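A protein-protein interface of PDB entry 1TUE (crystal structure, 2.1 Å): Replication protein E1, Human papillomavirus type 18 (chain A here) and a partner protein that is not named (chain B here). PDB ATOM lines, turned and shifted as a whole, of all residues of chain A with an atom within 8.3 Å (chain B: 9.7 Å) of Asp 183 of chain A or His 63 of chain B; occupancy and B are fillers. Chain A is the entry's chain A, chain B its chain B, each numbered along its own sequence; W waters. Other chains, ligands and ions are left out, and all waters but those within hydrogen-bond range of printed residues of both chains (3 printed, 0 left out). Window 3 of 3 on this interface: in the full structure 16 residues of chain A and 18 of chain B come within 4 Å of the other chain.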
ATOM      1  N   TYR A  36      33.609 -17.501 -18.568  1.00  0.00           N
ATOM      2  CA  TYR A  36      33.630 -18.799 -17.887  1.00  0.00           C
ATOM      3  C   TYR A  36      34.837 -18.920 -16.933  1.00  0.00           C
ATOM      4  O   TYR A  36      34.712 -19.468 -15.830  1.00  0.00           O
ATOM      5  CB  TYR A  36      33.616 -19.957 -18.889  1.00  0.00           C
ATOM      6  CG  TYR A  36      33.900 -21.309 -18.248  1.00  0.00           C
ATOM      7  CD1 TYR A  36      32.878 -22.055 -17.651  1.00  0.00           C
ATOM      8  CD2 TYR A  36      35.195 -21.836 -18.235  1.00  0.00           C
ATOM      9  CE1 TYR A  36      33.150 -23.286 -17.045  1.00  0.00           C
ATOM     10  CE2 TYR A  36      35.472 -23.055 -17.641  1.00  0.00           C
ATOM     11  CZ  TYR A  36      34.450 -23.779 -17.052  1.00  0.00           C
ATOM     12  OH  TYR A  36      34.731 -24.990 -16.458  1.00  0.00           O
ATOM     13  N   ASN A 178      39.087 -22.593 -13.839  1.00  0.00           N
ATOM     14  CA  ASN A 178      38.128 -23.647 -14.101  1.00  0.00           C
ATOM     15  C   ASN A 178      38.559 -24.617 -15.191  1.00  0.00           C
ATOM     16  O   ASN A 178      39.214 -24.217 -16.151  1.00  0.00           O
ATOM     17  CB  ASN A 178      36.750 -23.045 -14.380  1.00  0.00           C
ATOM     18  CG  ASN A 178      36.239 -22.193 -13.211  1.00  0.00           C
ATOM     19  OD1 ASN A 178      36.431 -22.545 -12.043  1.00  0.00           O
ATOM     20  ND2 ASN A 178      35.597 -21.064 -13.523  1.00  0.00           N
ATOM     21  N   ALA A 179      38.204 -25.894 -15.025  1.00  0.00           N
ATOM     22  CA  ALA A 179      38.533 -26.928 -16.021  1.00  0.00           C
ATOM     23  C   ALA A 179      37.855 -26.633 -17.357  1.00  0.00           C
ATOM     24  O   ALA A 179      36.746 -26.097 -17.384  1.00  0.00           O
ATOM     25  CB  ALA A 179      38.141 -28.307 -15.517  1.00  0.00           C
ATOM     26  N   PHE A 180      38.528 -26.960 -18.459  1.00  0.00           N
ATOM     27  CA  PHE A 180      37.965 -26.749 -19.793  1.00  0.00           C
ATOM     28  C   PHE A 180      36.650 -27.524 -19.849  1.00  0.00           C
ATOM     29  O   PHE A 180      36.637 -28.716 -19.567  1.00  0.00           O
ATOM     30  CB  PHE A 180      38.949 -27.216 -20.880  1.00  0.00           C
ATOM     31  CG  PHE A 180      38.600 -26.743 -22.274  1.00  0.00           C
ATOM     32  CD1 PHE A 180      38.818 -25.427 -22.654  1.00  0.00           C
ATOM     33  CD2 PHE A 180      38.090 -27.626 -23.211  1.00  0.00           C
ATOM     34  CE1 PHE A 180      38.510 -24.987 -23.949  1.00  0.00           C
ATOM     35  CE2 PHE A 180      37.773 -27.202 -24.504  1.00  0.00           C
ATOM     36  CZ  PHE A 180      37.994 -25.880 -24.875  1.00  0.00           C
ATOM     37  N   PRO A 181      35.536 -26.848 -20.138  1.00  0.00           N
ATOM     38  CA  PRO A 181      34.226 -27.495 -20.078  1.00  0.00           C
ATOM     39  C   PRO A 181      33.831 -28.292 -21.314  1.00  0.00           C
ATOM     40  O   PRO A 181      34.070 -27.857 -22.442  1.00  0.00           O
ATOM     41  CB  PRO A 181      33.258 -26.318 -19.866  1.00  0.00           C
ATOM     42  CG  PRO A 181      33.946 -25.141 -20.462  1.00  0.00           C
ATOM     43  CD  PRO A 181      35.431 -25.417 -20.481  1.00  0.00           C
ATOM     44  N   PHE A 182      33.216 -29.448 -21.071  1.00  0.00           N
ATOM     45  CA  PHE A 182      32.686 -30.339 -22.111  1.00  0.00           C
ATOM     46  C   PHE A 182      31.210 -30.609 -21.854  1.00  0.00           C
ATOM     47  O   PHE A 182      30.769 -30.615 -20.698  1.00  0.00           O
ATOM     48  CB  PHE A 182      33.426 -31.677 -22.102  1.00  0.00           C
ATOM     49  CG  PHE A 182      34.870 -31.578 -22.482  1.00  0.00           C
ATOM     50  CD1 PHE A 182      35.252 -31.595 -23.815  1.00  0.00           C
ATOM     51  CD2 PHE A 182      35.857 -31.492 -21.501  1.00  0.00           C
ATOM     52  CE1 PHE A 182      36.590 -31.497 -24.172  1.00  0.00           C
ATOM     53  CE2 PHE A 182      37.205 -31.410 -21.851  1.00  0.00           C
ATOM     54  CZ  PHE A 182      37.565 -31.407 -23.187  1.00  0.00           C
ATOM     55  N   ASP A 183      30.448 -30.842 -22.922  1.00  0.00           N
ATOM     56  CA  ASP A 183      29.023 -31.124 -22.772  1.00  0.00           C
ATOM     57  C   ASP A 183      28.768 -32.624 -22.550  1.00  0.00           C
ATOM     58  O   ASP A 183      29.715 -33.414 -22.461  1.00  0.00           O
ATOM     59  CB  ASP A 183      28.213 -30.551 -23.948  1.00  0.00           C
ATOM     60  CG  ASP A 183      28.475 -31.268 -25.266  1.00  0.00           C
ATOM     61  OD1 ASP A 183      28.943 -32.427 -25.260  1.00  0.00           O
ATOM     62  OD2 ASP A 183      28.222 -30.744 -26.372  1.00  0.00           O
ATOM     63  N   LYS A 184      27.496 -33.015 -22.478  1.00  0.00           N
ATOM     64  CA  LYS A 184      27.120 -34.404 -22.156  1.00  0.00           C
ATOM     65  C   LYS A 184      27.601 -35.464 -23.168  1.00  0.00           C
ATOM     66  O   LYS A 184      27.665 -36.655 -22.842  1.00  0.00           O
ATOM     67  CB  LYS A 184      25.600 -34.515 -21.910  1.00  0.00           C
ATOM     68  CG  LYS A 184      24.729 -34.530 -23.169  1.00  0.00           C
ATOM     69  CD  LYS A 184      23.311 -34.020 -22.886  1.00  0.00           C
ATOM     70  CE  LYS A 184      23.191 -32.527 -23.207  1.00  0.00           C
ATOM     71  NZ  LYS A 184      22.198 -31.806 -22.348  1.00  0.00           N
ATOM     72  N   ASN A 185      27.949 -35.024 -24.377  1.00  0.00           N
ATOM     73  CA  ASN A 185      28.450 -35.908 -25.427  1.00  0.00           C
ATOM     74  C   ASN A 185      29.977 -35.908 -25.544  1.00  0.00           C
ATOM     75  O   ASN A 185      30.546 -36.520 -26.458  1.00  0.00           O
ATOM     76  CB  ASN A 185      27.844 -35.516 -26.781  1.00  0.00           C
ATOM     77  CG  ASN A 185      26.334 -35.397 -26.736  1.00  0.00           C
ATOM     78  OD1 ASN A 185      25.656 -36.158 -26.041  1.00  0.00           O
ATOM     79  ND2 ASN A 185      25.795 -34.437 -27.481  1.00  0.00           N
ATOM     80  N   GLY A 186      30.640 -35.210 -24.630  1.00  0.00           N
ATOM     81  CA  GLY A 186      32.094 -35.106 -24.667  1.00  0.00           C
ATOM     82  C   GLY A 186      32.604 -34.078 -25.659  1.00  0.00           C
ATOM     83  O   GLY A 186      33.801 -34.038 -25.940  1.00  0.00           O
ATOM     84  N   ASN A 187      31.700 -33.254 -26.196  1.00  0.00           N
ATOM     85  CA  ASN A 187      32.076 -32.166 -27.102  1.00  0.00           C
ATOM     86  C   ASN A 187      32.393 -30.908 -26.283  1.00  0.00           C
ATOM     87  O   ASN A 187      31.694 -30.623 -25.312  1.00  0.00           O
ATOM     88  CB  ASN A 187      30.950 -31.864 -28.103  1.00  0.00           C
ATOM     89  CG  ASN A 187      30.771 -32.961 -29.158  1.00  0.00           C
ATOM     90  OD1 ASN A 187      31.743 -33.512 -29.675  1.00  0.00           O
ATOM     91  ND2 ASN A 187      29.518 -33.266 -29.487  1.00  0.00           N
ATOM     92  N   PRO A 188      33.446 -30.180 -26.656  1.00  0.00           N
ATOM     93  CA  PRO A 188      33.805 -28.932 -25.971  1.00  0.00           C
ATOM     94  C   PRO A 188      32.664 -27.920 -26.024  1.00  0.00           C
ATOM     95  O   PRO A 188      32.033 -27.742 -27.068  1.00  0.00           O
ATOM     96  CB  PRO A 188      34.999 -28.417 -26.783  1.00  0.00           C
ATOM     97  CG  PRO A 188      34.880 -29.107 -28.103  1.00  0.00           C
ATOM     98  CD  PRO A 188      34.381 -30.484 -27.757  1.00  0.00           C
ATOM     99  N   VAL A 189      32.394 -27.272 -24.904  1.00  0.00           N
ATOM    100  CA  VAL A 189      31.380 -26.233 -24.883  1.00  0.00           C
ATOM    101  C   VAL A 189      31.814 -25.051 -25.763  1.00  0.00           C
ATOM    102  O   VAL A 189      30.996 -24.470 -26.485  1.00  0.00           O
ATOM    103  CB  VAL A 189      31.021 -25.824 -23.431  1.00  0.00           C
ATOM    104  CG1 VAL A 189      29.995 -24.698 -23.401  1.00  0.00           C
ATOM    105  CG2 VAL A 189      30.473 -27.024 -22.686  1.00  0.00           C
ATOM    106  N   TYR A 190      33.107 -24.735 -25.733  1.00  0.00           N
ATOM    107  CA  TYR A 190      33.642 -23.605 -26.485  1.00  0.00           C
ATOM    108  C   TYR A 190      34.786 -24.048 -27.387  1.00  0.00           C
ATOM    109  O   TYR A 190      35.789 -24.562 -26.915  1.00  0.00           O
ATOM    110  CB  TYR A 190      34.149 -22.513 -25.543  1.00  0.00           C
ATOM    111  CG  TYR A 190      33.195 -22.141 -24.428  1.00  0.00           C
ATOM    112  CD1 TYR A 190      31.951 -21.552 -24.711  1.00  0.00           C
ATOM    113  CD2 TYR A 190      33.534 -22.366 -23.097  1.00  0.00           C
ATOM    114  CE1 TYR A 190      31.077 -21.224 -23.701  1.00  0.00           C
ATOM    115  CE2 TYR A 190      32.660 -22.028 -22.069  1.00  0.00           C
ATOM    116  CZ  TYR A 190      31.442 -21.454 -22.385  1.00  0.00           C
ATOM    117  OH  TYR A 190      30.580 -21.115 -21.386  1.00  0.00           O
ATOM    118  N   LYS B   8      16.747 -25.706 -11.544  1.00  0.00           N
ATOM    119  CA  LYS B   8      17.999 -25.519 -12.269  1.00  0.00           C
ATOM    120  C   LYS B   8      17.751 -25.141 -13.729  1.00  0.00           C
ATOM    121  O   LYS B   8      18.435 -24.270 -14.259  1.00  0.00           O
ATOM    122  CB  LYS B   8      18.885 -26.766 -12.172  1.00  0.00           C
ATOM    123  CG  LYS B   8      20.331 -26.509 -12.586  1.00  0.00           C
ATOM    124  CD  LYS B   8      21.155 -27.781 -12.595  1.00  0.00           C
ATOM    125  CE  LYS B   8      22.377 -27.607 -13.476  1.00  0.00           C
ATOM    126  NZ  LYS B   8      23.138 -28.868 -13.640  1.00  0.00           N
ATOM    127  N   SER B  12      18.733 -21.710 -15.380  1.00  0.00           N
ATOM    128  CA  SER B  12      19.545 -21.910 -16.583  1.00  0.00           C
ATOM    129  C   SER B  12      19.030 -21.124 -17.773  1.00  0.00           C
ATOM    130  O   SER B  12      19.803 -20.449 -18.457  1.00  0.00           O
ATOM    131  CB  SER B  12      19.582 -23.398 -16.938  1.00  0.00           C
ATOM    132  OG  SER B  12      19.789 -23.590 -18.330  1.00  0.00           O
ATOM    133  N   LEU B  15      19.655 -17.421 -17.063  1.00  0.00           N
ATOM    134  CA  LEU B  15      21.074 -17.068 -17.156  1.00  0.00           C
ATOM    135  C   LEU B  15      21.533 -17.009 -18.603  1.00  0.00           C
ATOM    136  O   LEU B  15      22.263 -16.103 -18.995  1.00  0.00           O
ATOM    137  CB  LEU B  15      21.945 -18.045 -16.363  1.00  0.00           C
ATOM    138  CG  LEU B  15      23.454 -17.779 -16.337  1.00  0.00           C
ATOM    139  CD1 LEU B  15      23.781 -16.589 -15.445  1.00  0.00           C
ATOM    140  CD2 LEU B  15      24.197 -19.022 -15.878  1.00  0.00           C
ATOM    141  N   SER B  16      21.098 -17.981 -19.395  1.00  0.00           N
ATOM    142  CA  SER B  16      21.459 -18.035 -20.809  1.00  0.00           C
ATOM    143  C   SER B  16      21.017 -16.784 -21.576  1.00  0.00           C
ATOM    144  O   SER B  16      21.750 -16.296 -22.431  1.00  0.00           O
ATOM    145  CB  SER B  16      20.901 -19.292 -21.462  1.00  0.00           C
ATOM    146  OG  SER B  16      21.320 -19.349 -22.811  1.00  0.00           O
ATOM    147  N   GLN B  19      23.246 -13.766 -20.193  1.00  0.00           N
ATOM    148  CA  GLN B  19      24.615 -13.830 -20.704  1.00  0.00           C
ATOM    149  C   GLN B  19      24.698 -13.528 -22.195  1.00  0.00           C
ATOM    150  O   GLN B  19      25.652 -12.900 -22.629  1.00  0.00           O
ATOM    151  CB  GLN B  19      25.277 -15.157 -20.345  1.00  0.00           C
ATOM    152  CG  GLN B  19      25.490 -15.291 -18.836  1.00  0.00           C
ATOM    153  CD  GLN B  19      26.296 -16.499 -18.443  1.00  0.00           C
ATOM    154  OE1 GLN B  19      26.250 -17.540 -19.115  1.00  0.00           O
ATOM    155  NE2 GLN B  19      27.040 -16.375 -17.345  1.00  0.00           N
ATOM    156  N   PHE B  50      23.335 -16.552  -9.897  1.00  0.00           N
ATOM    157  CA  PHE B  50      24.406 -17.395  -9.366  1.00  0.00           C
ATOM    158  C   PHE B  50      24.300 -17.565  -7.836  1.00  0.00           C
ATOM    159  O   PHE B  50      24.611 -18.635  -7.301  1.00  0.00           O
ATOM    160  CB  PHE B  50      25.783 -16.833  -9.750  1.00  0.00           C
ATOM    161  CG  PHE B  50      26.257 -17.224 -11.146  1.00  0.00           C
ATOM    162  CD1 PHE B  50      26.178 -18.541 -11.587  1.00  0.00           C
ATOM    163  CD2 PHE B  50      26.839 -16.275 -11.986  1.00  0.00           C
ATOM    164  CE1 PHE B  50      26.650 -18.914 -12.856  1.00  0.00           C
ATOM    165  CE2 PHE B  50      27.307 -16.625 -13.260  1.00  0.00           C
ATOM    166  CZ  PHE B  50      27.211 -17.951 -13.698  1.00  0.00           C
ATOM    167  N   ILE B  58      23.067 -25.904  -6.510  1.00  0.00           N
ATOM    168  CA  ILE B  58      23.472 -26.100  -7.900  1.00  0.00           C
ATOM    169  C   ILE B  58      24.968 -25.755  -8.071  1.00  0.00           C
ATOM    170  O   ILE B  58      25.400 -24.651  -7.739  1.00  0.00           O
ATOM    171  CB  ILE B  58      22.557 -25.272  -8.840  1.00  0.00           C
ATOM    172  CG1 ILE B  58      21.111 -25.790  -8.777  1.00  0.00           C
ATOM    173  CG2 ILE B  58      23.054 -25.310 -10.287  1.00  0.00           C
ATOM    174  CD1 ILE B  58      20.067 -24.750  -9.179  1.00  0.00           C
ATOM    175  N   GLN B  59      25.745 -26.716  -8.568  1.00  0.00           N
ATOM    176  CA  GLN B  59      27.204 -26.568  -8.693  1.00  0.00           C
ATOM    177  C   GLN B  59      27.612 -25.907 -10.002  1.00  0.00           C
ATOM    178  O   GLN B  59      28.543 -25.098 -10.038  1.00  0.00           O
ATOM    179  CB  GLN B  59      27.899 -27.932  -8.569  1.00  0.00           C
ATOM    180  CG  GLN B  59      29.382 -27.841  -8.176  1.00  0.00           C
ATOM    181  CD  GLN B  59      30.123 -29.169  -8.274  1.00  0.00           C
ATOM    182  OE1 GLN B  59      29.567 -30.173  -8.739  1.00  0.00           O
ATOM    183  NE2 GLN B  59      31.381 -29.175  -7.850  1.00  0.00           N
ATOM    184  N   THR B  60      26.932 -26.277 -11.084  1.00  0.00           N
ATOM    185  CA  THR B  60      27.185 -25.667 -12.387  1.00  0.00           C
ATOM    186  C   THR B  60      25.865 -25.339 -13.068  1.00  0.00           C
ATOM    187  O   THR B  60      24.881 -26.059 -12.909  1.00  0.00           O
ATOM    188  CB  THR B  60      28.067 -26.568 -13.305  1.00  0.00           C
ATOM    189  OG1 THR B  60      27.315 -27.692 -13.746  1.00  0.00           O
ATOM    190  CG2 THR B  60      29.211 -27.211 -12.538  1.00  0.00           C
ATOM    191  N   LEU B  61      25.859 -24.259 -13.840  1.00  0.00           N
ATOM    192  CA  LEU B  61      24.649 -23.759 -14.449  1.00  0.00           C
ATOM    193  C   LEU B  61      24.993 -23.357 -15.872  1.00  0.00           C
ATOM    194  O   LEU B  61      25.836 -22.490 -16.080  1.00  0.00           O
ATOM    195  CB  LEU B  61      24.178 -22.531 -13.670  1.00  0.00           C
ATOM    196  CG  LEU B  61      22.753 -22.365 -13.154  1.00  0.00           C
ATOM    197  CD1 LEU B  61      22.452 -20.886 -13.029  1.00  0.00           C
ATOM    198  CD2 LEU B  61      21.705 -23.061 -14.019  1.00  0.00           C
ATOM    199  N   ASN B  62      24.349 -23.980 -16.856  1.00  0.00           N
ATOM    200  CA  ASN B  62      24.710 -23.759 -18.265  1.00  0.00           C
ATOM    201  C   ASN B  62      26.219 -23.879 -18.466  1.00  0.00           C
ATOM    202  O   ASN B  62      26.850 -23.017 -19.091  1.00  0.00           O
ATOM    203  CB  ASN B  62      24.232 -22.388 -18.753  1.00  0.00           C
ATOM    204  CG  ASN B  62      22.730 -22.251 -18.734  1.00  0.00           C
ATOM    205  OD1 ASN B  62      21.995 -23.246 -18.813  1.00  0.00           O
ATOM    206  ND2 ASN B  62      22.255 -21.013 -18.646  1.00  0.00           N
ATOM    207  N   HIS B  63      26.783 -24.941 -17.898  1.00  0.00           N
ATOM    208  CA  HIS B  63      28.225 -25.214 -17.929  1.00  0.00           C
ATOM    209  C   HIS B  63      29.087 -24.250 -17.115  1.00  0.00           C
ATOM    210  O   HIS B  63      30.273 -24.510 -16.925  1.00  0.00           O
ATOM    211  CB  HIS B  63      28.753 -25.301 -19.372  1.00  0.00           C
ATOM    212  CG  HIS B  63      27.978 -26.239 -20.235  1.00  0.00           C
ATOM    213  ND1 HIS B  63      28.025 -27.605 -20.072  1.00  0.00           N
ATOM    214  CD2 HIS B  63      27.123 -26.007 -21.258  1.00  0.00           C
ATOM    215  CE1 HIS B  63      27.233 -28.176 -20.963  1.00  0.00           C
ATOM    216  NE2 HIS B  63      26.673 -27.228 -21.692  1.00  0.00           N
ATOM    217  N   GLN B  64      28.501 -23.150 -16.644  1.00  0.00           N
ATOM    218  CA  GLN B  64      29.234 -22.171 -15.831  1.00  0.00           C
ATOM    219  C   GLN B  64      29.414 -22.696 -14.418  1.00  0.00           C
ATOM    220  O   GLN B  64      28.481 -23.240 -13.826  1.00  0.00           O
ATOM    221  CB  GLN B  64      28.512 -20.811 -15.795  1.00  0.00           C
ATOM    222  CG  GLN B  64      28.082 -20.292 -17.176  1.00  0.00           C
ATOM    223  CD  GLN B  64      29.235 -20.226 -18.170  1.00  0.00           C
ATOM    224  OE1 GLN B  64      30.144 -19.404 -18.028  1.00  0.00           O
ATOM    225  NE2 GLN B  64      29.205 -21.101 -19.174  1.00  0.00           N
ATOM    226  N   VAL B  65      30.613 -22.523 -13.878  1.00  0.00           N
ATOM    227  CA  VAL B  65      30.873 -22.885 -12.494  1.00  0.00           C
ATOM    228  C   VAL B  65      30.241 -21.813 -11.592  1.00  0.00           C
ATOM    229  O   VAL B  65      30.588 -20.626 -11.669  1.00  0.00           O
ATOM    230  CB  VAL B  65      32.394 -23.065 -12.220  1.00  0.00           C
ATOM    231  CG1 VAL B  65      32.639 -23.464 -10.773  1.00  0.00           C
ATOM    232  CG2 VAL B  65      32.995 -24.126 -13.155  1.00  0.00           C
ATOM    233  N   VAL B  66      29.286 -22.230 -10.762  1.00  0.00           N
ATOM    234  CA  VAL B  66      28.590 -21.310  -9.859  1.00  0.00           C
ATOM    235  C   VAL B  66      29.613 -20.816  -8.842  1.00  0.00           C
ATOM    236  O   VAL B  66      30.189 -21.635  -8.121  1.00  0.00           O
ATOM    237  CB  VAL B  66      27.388 -22.010  -9.150  1.00  0.00           C
ATOM    238  CG1 VAL B  66      26.750 -21.106  -8.074  1.00  0.00           C
ATOM    239  CG2 VAL B  66      26.347 -22.448 -10.159  1.00  0.00           C
ATOM    240  N   PRO B  67      29.858 -19.498  -8.776  1.00  0.00           N
ATOM    241  CA  PRO B  67      30.901 -18.980  -7.898  1.00  0.00           C
ATOM    242  C   PRO B  67      30.526 -19.075  -6.421  1.00  0.00           C
ATOM    243  O   PRO B  67      29.369 -19.318  -6.075  1.00  0.00           O
ATOM    244  CB  PRO B  67      31.035 -17.498  -8.321  1.00  0.00           C
ATOM    245  CG  PRO B  67      30.205 -17.354  -9.587  1.00  0.00           C
ATOM    246  CD  PRO B  67      29.165 -18.413  -9.498  1.00  0.00           C
HETATM  247  O   HOH W   1      32.118 -20.422 -14.929  1.00  0.00           O
HETATM  248  O   HOH W   2      29.899 -28.718 -18.873  1.00  0.00           O
HETATM  249  O   HOH W   3      33.689 -19.631 -11.754  1.00  0.00           O
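The side-chain amide nitrogen (NE2) of Gln 64 of chain B lies within hydrogen-bond range of the side-chain hydroxyl (OH) of Tyr 190 of chain A (2.6 Å).
The backbone carbonyl oxygen of Ala 179 of chain A sits at hydrogen-bond distance from the side-chain hydroxyl of Tyr 36 of chain A, at 2.5 Å.
The backbone carbonyl oxygen (O) of Pro 181 of chain A lies within hydrogen-bond range of the backbone NH (N) of Val 189 of chain A, 3.0 Å away.
The backbone NH (N) of Asn 185 of chain A is in hydrogen-bond range of the side-chain carboxylate (OD1) of Asp 183 of chain A, at 2.9 Å.
OD1 of Asp 183 of chain A is in hydrogen-bond range of N of Gly 186 of chain A, at 3.3 Å.
The side-chain carboxylate of Asp 183 of chain A lies within hydrogen-bond range of the backbone NH of Asn 187 of chain A (3.0 Å).
The backbone carbonyl oxygen (O) of Asn 62 of chain B is in hydrogen-bond range of the side-chain amide nitrogen (NE2) of Gln 64 of chain B, 3.0 Å away.
Tyr 36 of chain A touches His 63 of chain B.
Tyr 36 of chain A touches Gln 64 of chain B.
Tyr 36 of chain A touches Val 65 of chain B (OH to CG2, 3.8 Å).
Asn 178 of chain A touches Val 65 of chain B.
Asp 183 of chain A touches His 63 of chain B (CA to CE1, 3.9 Å).
CG2 of Val 189 of chain A touches CG of His 63 of chain B (3.6 Å).
Printed residues of chain B within 4 Å of Asp 183 of chain A: His 63.
No residue of chain B comes within 4 Å of Asn 185 of chain A.
No residue of chain B comes within 4 Å of Gly 186 of chain A.
No residue of chain B comes within 4 Å of Asn 187 of chain A.
Of the printed residues of chain B, Asn 178 of chain A touches Val 65 (3.8 Å).
Of the printed residues of chain A, Val 65 of chain B touches Tyr 36 and Asn 178.
Phe 182 of chain A touches none of the printed residues of chain B.
Val 66 of chain B touches none of the printed residues of chain A.
The nearest residue of chain B that does not touch Asp 183 of chain A is Asn 62 of chain B (8.9 Å).
The nearest printed residue of chain B that does not touch Asn 178 of chain A is Gln 64 of chain B (6.5 Å).
Of the 16 printed residues of chain B, 3 touch a printed residue of chain A.
Along chain A the printed residues that touch a printed residue of chain B span positions 36 to 190.
Among the printed residues, 7 pairs touch across the chains.
Among the printed residues, no Asp or Glu carboxylate lies within 4 Å of a Lys or Arg side-chain nitrogen of the other chain.
Water W2 lies within hydrogen-bond range of ND1 of His 63 of chain B (2.5 Å) and O of Phe 182 of chain A (2.8 Å).
Water W1 bridges N of Val 65 of chain B and O of Tyr 36 of chain A.
Water W3 bridges ND2 of Asn 178 of chain A (3.0 Å) and O of Val 65 of chain B (3.3 Å).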
